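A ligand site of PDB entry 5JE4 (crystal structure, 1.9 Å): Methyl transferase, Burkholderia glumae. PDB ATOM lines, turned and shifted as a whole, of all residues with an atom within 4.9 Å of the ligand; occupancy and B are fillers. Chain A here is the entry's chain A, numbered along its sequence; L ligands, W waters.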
ATOM      1  N   ARG A  26     -27.619  29.041  -0.507  1.00  0.00           N
ATOM      2  CA  ARG A  26     -26.895  29.436  -1.716  1.00  0.00           C
ATOM      3  C   ARG A  26     -25.486  29.927  -1.384  1.00  0.00           C
ATOM      4  O   ARG A  26     -24.533  29.632  -2.123  1.00  0.00           O
ATOM      5  CB  ARG A  26     -27.669  30.491  -2.502  1.00  0.00           C
ATOM      6  CG  ARG A  26     -27.244  30.613  -3.972  1.00  0.00           C
ATOM      7  CD  ARG A  26     -28.316  30.062  -4.954  1.00  0.00           C
ATOM      8  NE  ARG A  26     -27.869  28.888  -5.717  1.00  0.00           N
ATOM      9  CZ  ARG A  26     -27.723  28.856  -7.046  1.00  0.00           C
ATOM     10  NH1 ARG A  26     -27.988  29.930  -7.782  1.00  0.00           N
ATOM     11  NH2 ARG A  26     -27.326  27.734  -7.649  1.00  0.00           N
ATOM     12  N   GLU A  29     -23.328  26.877  -0.962  1.00  0.00           N
ATOM     13  CA  GLU A  29     -23.131  26.221  -2.249  1.00  0.00           C
ATOM     14  C   GLU A  29     -22.104  26.989  -3.091  1.00  0.00           C
ATOM     15  O   GLU A  29     -21.213  26.391  -3.715  1.00  0.00           O
ATOM     16  CB  GLU A  29     -24.457  26.120  -2.989  1.00  0.00           C
ATOM     17  CG  GLU A  29     -24.352  26.187  -4.494  1.00  0.00           C
ATOM     18  CD  GLU A  29     -25.700  26.073  -5.172  1.00  0.00           C
ATOM     19  OE1 GLU A  29     -26.740  26.296  -4.512  1.00  0.00           O
ATOM     20  OE2 GLU A  29     -25.730  25.771  -6.380  1.00  0.00           O
ATOM     21  N   LEU A  48     -22.335  23.682 -17.619  1.00  0.00           N
ATOM     22  CA  LEU A  48     -23.430  22.816 -18.048  1.00  0.00           C
ATOM     23  C   LEU A  48     -24.649  22.997 -17.159  1.00  0.00           C
ATOM     24  O   LEU A  48     -24.533  23.196 -15.941  1.00  0.00           O
ATOM     25  CB  LEU A  48     -22.998  21.354 -18.024  1.00  0.00           C
ATOM     26  CG  LEU A  48     -21.860  20.974 -18.958  1.00  0.00           C
ATOM     27  CD1 LEU A  48     -21.587  19.490 -18.845  1.00  0.00           C
ATOM     28  CD2 LEU A  48     -22.234  21.358 -20.399  1.00  0.00           C
ATOM     29  N   ALA A  49     -25.835  22.849 -17.756  1.00  0.00           N
ATOM     30  CA  ALA A  49     -27.097  23.164 -17.066  1.00  0.00           C
ATOM     31  C   ALA A  49     -27.025  24.579 -16.498  1.00  0.00           C
ATOM     32  O   ALA A  49     -27.347  24.821 -15.325  1.00  0.00           O
ATOM     33  CB  ALA A  49     -27.424  22.146 -15.971  1.00  0.00           C
ATOM     34  N   CYS A  50     -26.623  25.528 -17.346  1.00  0.00           N
ATOM     35  CA  CYS A  50     -26.193  26.822 -16.856  1.00  0.00           C
ATOM     36  C   CYS A  50     -27.327  27.724 -16.385  1.00  0.00           C
ATOM     37  O   CYS A  50     -27.038  28.716 -15.701  1.00  0.00           O
ATOM     38  CB  CYS A  50     -25.366  27.550 -17.929  1.00  0.00           C
ATOM     39  SG  CYS A  50     -26.312  28.016 -19.410  1.00  0.00           S
ATOM     40  N   GLY A  51     -28.585  27.429 -16.723  1.00  0.00           N
ATOM     41  CA  GLY A  51     -29.658  28.341 -16.358  1.00  0.00           C
ATOM     42  C   GLY A  51     -29.427  29.709 -16.977  1.00  0.00           C
ATOM     43  O   GLY A  51     -29.087  29.817 -18.163  1.00  0.00           O
ATOM     44  N   PHE A  54     -25.456  31.911 -13.962  1.00  0.00           N
ATOM     45  CA  PHE A  54     -24.909  32.443 -12.722  1.00  0.00           C
ATOM     46  C   PHE A  54     -23.458  32.019 -12.496  1.00  0.00           C
ATOM     47  O   PHE A  54     -22.578  32.860 -12.268  1.00  0.00           O
ATOM     48  CB  PHE A  54     -25.766  32.022 -11.526  1.00  0.00           C
ATOM     49  CG  PHE A  54     -25.196  32.442 -10.206  1.00  0.00           C
ATOM     50  CD1 PHE A  54     -25.338  33.750  -9.760  1.00  0.00           C
ATOM     51  CD2 PHE A  54     -24.492  31.542  -9.420  1.00  0.00           C
ATOM     52  CE1 PHE A  54     -24.800  34.148  -8.552  1.00  0.00           C
ATOM     53  CE2 PHE A  54     -23.945  31.938  -8.212  1.00  0.00           C
ATOM     54  CZ  PHE A  54     -24.098  33.243  -7.775  1.00  0.00           C
ATOM     55  N   PHE A  55     -23.174  30.708 -12.560  1.00  0.00           N
ATOM     56  CA  PHE A  55     -21.831  30.248 -12.212  1.00  0.00           C
ATOM     57  C   PHE A  55     -20.831  30.569 -13.304  1.00  0.00           C
ATOM     58  O   PHE A  55     -19.725  31.028 -13.001  1.00  0.00           O
ATOM     59  CB  PHE A  55     -21.844  28.751 -11.889  1.00  0.00           C
ATOM     60  CG  PHE A  55     -22.329  28.471 -10.520  1.00  0.00           C
ATOM     61  CD1 PHE A  55     -21.530  28.748  -9.441  1.00  0.00           C
ATOM     62  CD2 PHE A  55     -23.611  28.005 -10.314  1.00  0.00           C
ATOM     63  CE1 PHE A  55     -21.989  28.535  -8.146  1.00  0.00           C
ATOM     64  CE2 PHE A  55     -24.080  27.798  -9.032  1.00  0.00           C
ATOM     65  CZ  PHE A  55     -23.262  28.069  -7.954  1.00  0.00           C
ATOM     66  N   VAL A  70     -24.262  25.968 -21.456  1.00  0.00           N
ATOM     67  CA  VAL A  70     -25.183  25.061 -22.143  1.00  0.00           C
ATOM     68  C   VAL A  70     -26.370  24.774 -21.248  1.00  0.00           C
ATOM     69  O   VAL A  70     -26.201  24.411 -20.077  1.00  0.00           O
ATOM     70  CB  VAL A  70     -24.501  23.736 -22.523  1.00  0.00           C
ATOM     71  CG1 VAL A  70     -25.523  22.759 -23.152  1.00  0.00           C
ATOM     72  CG2 VAL A  70     -23.339  23.981 -23.469  1.00  0.00           C
ATOM     73  N   ASP A  71     -27.575  24.916 -21.798  1.00  0.00           N
ATOM     74  CA  ASP A  71     -28.803  24.524 -21.117  1.00  0.00           C
ATOM     75  C   ASP A  71     -29.766  23.957 -22.151  1.00  0.00           C
ATOM     76  O   ASP A  71     -29.733  24.336 -23.332  1.00  0.00           O
ATOM     77  CB  ASP A  71     -29.430  25.726 -20.378  1.00  0.00           C
ATOM     78  CG  ASP A  71     -30.415  25.312 -19.290  1.00  0.00           C
ATOM     79  OD1 ASP A  71     -30.060  25.445 -18.097  1.00  0.00           O
ATOM     80  OD2 ASP A  71     -31.531  24.858 -19.606  1.00  0.00           O
ATOM     81  N   ILE A  72     -30.627  23.036 -21.711  1.00  0.00           N
ATOM     82  CA  ILE A  72     -31.590  22.417 -22.625  1.00  0.00           C
ATOM     83  C   ILE A  72     -32.778  23.327 -22.901  1.00  0.00           C
ATOM     84  O   ILE A  72     -33.509  23.082 -23.859  1.00  0.00           O
ATOM     85  CB  ILE A  72     -32.058  21.070 -22.060  1.00  0.00           C
ATOM     86  CG1 ILE A  72     -32.704  20.206 -23.133  1.00  0.00           C
ATOM     87  CG2 ILE A  72     -33.018  21.268 -20.879  1.00  0.00           C
ATOM     88  CD1 ILE A  72     -33.076  18.839 -22.615  1.00  0.00           C
ATOM     89  N   SER A  73     -32.980  24.368 -22.096  1.00  0.00           N
ATOM     90  CA  SER A  73     -34.124  25.262 -22.239  1.00  0.00           C
ATOM     91  C   SER A  73     -33.762  26.473 -23.103  1.00  0.00           C
ATOM     92  O   SER A  73     -32.831  27.220 -22.777  1.00  0.00           O
ATOM     93  CB  SER A  73     -34.599  25.736 -20.865  1.00  0.00           C
ATOM     94  OG  SER A  73     -35.417  26.886 -20.972  1.00  0.00           O
ATOM     95  N   MET A  76     -34.325  29.528 -20.923  1.00  0.00           N
ATOM     96  CA  MET A  76     -33.204  29.835 -20.037  1.00  0.00           C
ATOM     97  C   MET A  76     -32.046  30.466 -20.796  1.00  0.00           C
ATOM     98  O   MET A  76     -31.424  31.418 -20.311  1.00  0.00           O
ATOM     99  CB  MET A  76     -32.744  28.570 -19.307  1.00  0.00           C
ATOM    100  CG  MET A  76     -33.728  28.094 -18.252  1.00  0.00           C
ATOM    101  SD  MET A  76     -34.010  29.322 -16.966  1.00  0.00           S
ATOM    102  CE  MET A  76     -33.840  28.301 -15.487  1.00  0.00           C
ATOM    103  N   ARG A  96     -28.578  22.967 -25.767  1.00  0.00           N
ATOM    104  CA  ARG A  96     -28.302  21.557 -26.044  1.00  0.00           C
ATOM    105  C   ARG A  96     -28.777  20.699 -24.884  1.00  0.00           C
ATOM    106  O   ARG A  96     -28.841  21.154 -23.742  1.00  0.00           O
ATOM    107  CB  ARG A  96     -26.814  21.301 -26.290  1.00  0.00           C
ATOM    108  CG  ARG A  96     -26.303  21.604 -27.705  1.00  0.00           C
ATOM    109  CD  ARG A  96     -24.910  22.185 -27.587  1.00  0.00           C
ATOM    110  NE  ARG A  96     -24.105  22.213 -28.806  1.00  0.00           N
ATOM    111  CZ  ARG A  96     -24.297  23.047 -29.816  1.00  0.00           C
ATOM    112  NH1 ARG A  96     -25.307  23.911 -29.813  1.00  0.00           N
ATOM    113  NH2 ARG A  96     -23.474  22.998 -30.856  1.00  0.00           N
ATOM    114  N   ASP A  97     -29.094  19.442 -25.194  1.00  0.00           N
ATOM    115  CA  ASP A  97     -29.343  18.418 -24.186  1.00  0.00           C
ATOM    116  C   ASP A  97     -28.004  17.771 -23.874  1.00  0.00           C
ATOM    117  O   ASP A  97     -27.399  17.124 -24.739  1.00  0.00           O
ATOM    118  CB  ASP A  97     -30.353  17.393 -24.702  1.00  0.00           C
ATOM    119  CG  ASP A  97     -30.582  16.229 -23.742  1.00  0.00           C
ATOM    120  OD1 ASP A  97     -30.085  16.245 -22.591  1.00  0.00           O
ATOM    121  OD2 ASP A  97     -31.289  15.294 -24.145  1.00  0.00           O
ATOM    122  N   VAL A  98     -27.531  17.943 -22.637  1.00  0.00           N
ATOM    123  CA  VAL A  98     -26.202  17.468 -22.264  1.00  0.00           C
ATOM    124  C   VAL A  98     -26.095  15.961 -22.437  1.00  0.00           C
ATOM    125  O   VAL A  98     -25.033  15.442 -22.801  1.00  0.00           O
ATOM    126  CB  VAL A  98     -25.873  17.901 -20.835  1.00  0.00           C
ATOM    127  CG1 VAL A  98     -24.696  17.091 -20.281  1.00  0.00           C
ATOM    128  CG2 VAL A  98     -25.574  19.395 -20.797  1.00  0.00           C
ATOM    129  N   ALA A  99     -27.192  15.231 -22.200  1.00  0.00           N
ATOM    130  CA  ALA A  99     -27.152  13.779 -22.357  1.00  0.00           C
ATOM    131  C   ALA A  99     -26.932  13.374 -23.813  1.00  0.00           C
ATOM    132  O   ALA A  99     -26.357  12.307 -24.081  1.00  0.00           O
ATOM    133  CB  ALA A  99     -28.445  13.151 -21.836  1.00  0.00           C
ATOM    134  N   ALA A 113     -23.374  22.687 -11.913  1.00  0.00           N
ATOM    135  CA  ALA A 113     -24.176  22.926 -10.723  1.00  0.00           C
ATOM    136  C   ALA A 113     -25.622  22.596 -11.054  1.00  0.00           C
ATOM    137  O   ALA A 113     -26.278  23.332 -11.805  1.00  0.00           O
ATOM    138  CB  ALA A 113     -24.037  24.370 -10.250  1.00  0.00           C
ATOM    139  N   TRP A 114     -26.133  21.495 -10.494  1.00  0.00           N
ATOM    140  CA  TRP A 114     -27.517  21.061 -10.650  1.00  0.00           C
ATOM    141  C   TRP A 114     -27.789  20.613 -12.095  1.00  0.00           C
ATOM    142  O   TRP A 114     -28.786  20.977 -12.717  1.00  0.00           O
ATOM    143  CB  TRP A 114     -28.502  22.156 -10.206  1.00  0.00           C
ATOM    144  CG  TRP A 114     -28.213  22.596  -8.784  1.00  0.00           C
ATOM    145  CD1 TRP A 114     -27.832  23.842  -8.361  1.00  0.00           C
ATOM    146  CD2 TRP A 114     -28.292  21.774  -7.608  1.00  0.00           C
ATOM    147  NE1 TRP A 114     -27.652  23.844  -6.992  1.00  0.00           N
ATOM    148  CE2 TRP A 114     -27.940  22.593  -6.509  1.00  0.00           C
ATOM    149  CE3 TRP A 114     -28.627  20.434  -7.372  1.00  0.00           C
ATOM    150  CZ2 TRP A 114     -27.915  22.104  -5.198  1.00  0.00           C
ATOM    151  CZ3 TRP A 114     -28.591  19.954  -6.080  1.00  0.00           C
ATOM    152  CH2 TRP A 114     -28.234  20.791  -5.007  1.00  0.00           C
ATOM    153  N   LEU A 115     -26.869  19.807 -12.614  1.00  0.00           N
ATOM    154  CA  LEU A 115     -27.085  19.089 -13.872  1.00  0.00           C
ATOM    155  C   LEU A 115     -27.553  17.652 -13.627  1.00  0.00           C
ATOM    156  O   LEU A 115     -28.611  17.245 -14.120  1.00  0.00           O
ATOM    157  CB  LEU A 115     -25.788  19.060 -14.696  1.00  0.00           C
ATOM    158  CG  LEU A 115     -25.753  18.039 -15.851  1.00  0.00           C
ATOM    159  CD1 LEU A 115     -26.748  18.448 -16.918  1.00  0.00           C
ATOM    160  CD2 LEU A 115     -24.349  17.878 -16.469  1.00  0.00           C
ATOM    161  N   TYR A 118     -31.024  16.158 -12.851  1.00  0.00           N
ATOM    162  CA  TYR A 118     -32.087  16.213 -13.841  1.00  0.00           C
ATOM    163  C   TYR A 118     -31.979  15.101 -14.869  1.00  0.00           C
ATOM    164  O   TYR A 118     -32.808  15.049 -15.784  1.00  0.00           O
ATOM    165  CB  TYR A 118     -32.114  17.595 -14.518  1.00  0.00           C
ATOM    166  CG  TYR A 118     -32.517  18.625 -13.500  1.00  0.00           C
ATOM    167  CD1 TYR A 118     -33.827  18.712 -13.076  1.00  0.00           C
ATOM    168  CD2 TYR A 118     -31.568  19.425 -12.883  1.00  0.00           C
ATOM    169  CE1 TYR A 118     -34.205  19.621 -12.095  1.00  0.00           C
ATOM    170  CE2 TYR A 118     -31.927  20.326 -11.889  1.00  0.00           C
ATOM    171  CZ  TYR A 118     -33.244  20.431 -11.512  1.00  0.00           C
ATOM    172  OH  TYR A 118     -33.602  21.335 -10.532  1.00  0.00           O
ATOM    173  N   MET A 128     -24.488  11.579 -19.542  1.00  0.00           N
ATOM    174  CA  MET A 128     -24.011  12.909 -19.160  1.00  0.00           C
ATOM    175  C   MET A 128     -22.545  12.862 -18.735  1.00  0.00           C
ATOM    176  O   MET A 128     -21.738  13.699 -19.155  1.00  0.00           O
ATOM    177  CB  MET A 128     -24.876  13.480 -18.038  1.00  0.00           C
ATOM    178  CG  MET A 128     -26.290  13.849 -18.467  1.00  0.00           C
ATOM    179  SD  MET A 128     -27.119  14.643 -17.073  1.00  0.00           S
ATOM    180  CE  MET A 128     -28.723  15.016 -17.776  1.00  0.00           C
HETATM  181  N1  LIG L   1     -26.491  25.961 -13.033  1.00  0.00           N
HETATM  182  C1  LIG L   1     -27.571  26.982 -12.835  1.00  0.00           C
HETATM  183  C2  LIG L   1     -28.979  26.456 -13.145  1.00  0.00           C
HETATM  184  C3  LIG L   1     -29.407  25.214 -12.366  1.00  0.00           C
HETATM  185  S1  LIG L   1     -31.139  24.882 -12.591  1.00  0.00           S
HETATM  186  C4  LIG L   1     -27.515  27.485 -11.424  1.00  0.00           C
HETATM  187  O1  LIG L   1     -28.024  28.556 -11.126  1.00  0.00           O
HETATM  188  O2  LIG L   1     -26.955  26.828 -10.543  1.00  0.00           O
HETATM  189  C5  LIG L   1     -31.079  23.372 -13.507  1.00  0.00           C
HETATM  190  C6  LIG L   1     -30.995  23.690 -15.001  1.00  0.00           C
HETATM  191  O3  LIG L   1     -30.569  22.546 -15.730  1.00  0.00           O
HETATM  192  C7  LIG L   1     -32.286  24.164 -15.662  1.00  0.00           C
HETATM  193  O4  LIG L   1     -32.014  25.422 -16.317  1.00  0.00           O
HETATM  194  C8  LIG L   1     -32.585  23.128 -16.729  1.00  0.00           C
HETATM  195  O5  LIG L   1     -33.134  23.692 -17.929  1.00  0.00           O
HETATM  196  C9  LIG L   1     -31.204  22.542 -17.002  1.00  0.00           C
HETATM  197  N2  LIG L   1     -31.255  21.158 -17.535  1.00  0.00           N
HETATM  198  C10 LIG L   1     -32.046  20.156 -17.095  1.00  0.00           C
HETATM  199  N3  LIG L   1     -31.817  19.011 -17.790  1.00  0.00           N
HETATM  200  C11 LIG L   1     -30.859  19.303 -18.707  1.00  0.00           C
HETATM  201  C12 LIG L   1     -30.134  18.558 -19.755  1.00  0.00           C
HETATM  202  N4  LIG L   1     -30.417  17.261 -19.986  1.00  0.00           N
HETATM  203  N5  LIG L   1     -29.194  19.223 -20.473  1.00  0.00           N
HETATM  204  C13 LIG L   1     -28.913  20.514 -20.251  1.00  0.00           C
HETATM  205  N6  LIG L   1     -29.531  21.248 -19.305  1.00  0.00           N
HETATM  206  C14 LIG L   1     -30.484  20.709 -18.520  1.00  0.00           C
HETATM  207  O   HOH W   1     -28.145  30.586 -13.336  1.00  0.00           O
HETATM  208  O   HOH W   2     -23.886  24.699 -13.691  1.00  0.00           O
HETATM  209  O   HOH W   3     -24.816  28.352 -13.883  1.00  0.00           O
HETATM  210  O   HOH W   4     -35.615  22.328 -18.374  1.00  0.00           O
HETATM  211  O   HOH W   5     -32.693  15.889 -18.259  1.00  0.00           O
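An oxygen (O5) of the ligand sits at hydrogen-bond distance from the side-chain carboxylate (OD2) of Asp 71 (2.6 Å).
The backbone carbonyl oxygen (O) of Ala 49 lies within hydrogen-bond range of a nitrogen (N1) of the ligand (2.7 Å).
The side-chain carboxylate of Asp 97 is in hydrogen-bond range of a nitrogen (N4) of the ligand (2.8 Å).
The backbone carbonyl oxygen of Ala 113 sits at hydrogen-bond distance from a nitrogen (N1) of the ligand, at 2.9 Å.
N of Val 98 is in hydrogen-bond range of N5 of the ligand (3.0 Å).
An oxygen (O2) of the ligand lies within salt-bridge range of the guanidinium group (NH2) of Arg 26.
A nitrogen (N6) of the ligand is in hydrogen-bond range of the backbone NH of Ile 72 (3.2 Å).
The backbone NH (N) of Arg 96 lies within hydrogen-bond range of the backbone carbonyl oxygen (O) of Asp 71 (3.0 Å).
The side-chain carboxylate (OD1) of Asp 71 sits at hydrogen-bond distance from the backbone NH (N) of Gly 51 (2.8 Å).
The side-chain carboxylate (OD2) of Asp 71 lies within hydrogen-bond range of the backbone NH (N) of Ser 73.
The backbone carbonyl oxygen of Val 70 sits at hydrogen-bond distance from the backbone NH of Ala 49.
The guanidinium group (NH2) of Arg 26 lies within salt-bridge range of the side-chain carboxylate (OE2) of Glu 29 (2.8 Å).
The backbone NH (N) of Ile 72 sits close to the backbone carbonyl oxygen (O) of Arg 96 (3.3 Å).
The backbone carbonyl oxygen (O) of Val 70 is in hydrogen-bond range of the backbone NH (N) of Cys 50, 3.0 Å away.
N of Met 76 is in hydrogen-bond range of OG of Ser 73 (2.9 Å).
Cys 50 touches the ligand (O to C1, 3.4 Å).
Gly 51 touches the ligand.
Phe 55 touches the ligand.
CB of Ser 73 touches O5 of the ligand, at 3.9 Å.
Met 76 touches the ligand (CE to O4, 3.5 Å).
Arg 96 touches the ligand.
Trp 114 touches the ligand (O to C5, 3.4 Å).
Tyr 118 touches the ligand.
CE of Met 128 touches N4 of the ligand, at 3.6 Å.
Hydrophobic or aromatic side chains that line the ligand: Ala 49, Phe 55, Ile 72, Met 76, Val 98, Ala 113, Trp 114, Tyr 118 and Met 128.
Of the 22 residues printed, 16 come within 4 Å of the ligand.
Water W2 lies within hydrogen-bond range of N of Ala 113 (2.7 Å), O of Leu 48 (2.8 Å) and N1 of the ligand (3.0 Å).
Water W1 lies within hydrogen-bond range of an oxygen (O1) of the ligand (3.0 Å), the backbone NH (N) of Phe 54 (3.1 Å) and the backbone carbonyl oxygen (O) of Cys 50 (3.2 Å).
Water W3 lies within hydrogen-bond range of O of Cys 50 (2.9 Å), N1 of the ligand (3.0 Å) and N of Phe 55 (3.2 Å).
Water W5 lies within hydrogen-bond range of O of Tyr 118 (2.6 Å) and N4 of the ligand (3.2 Å).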
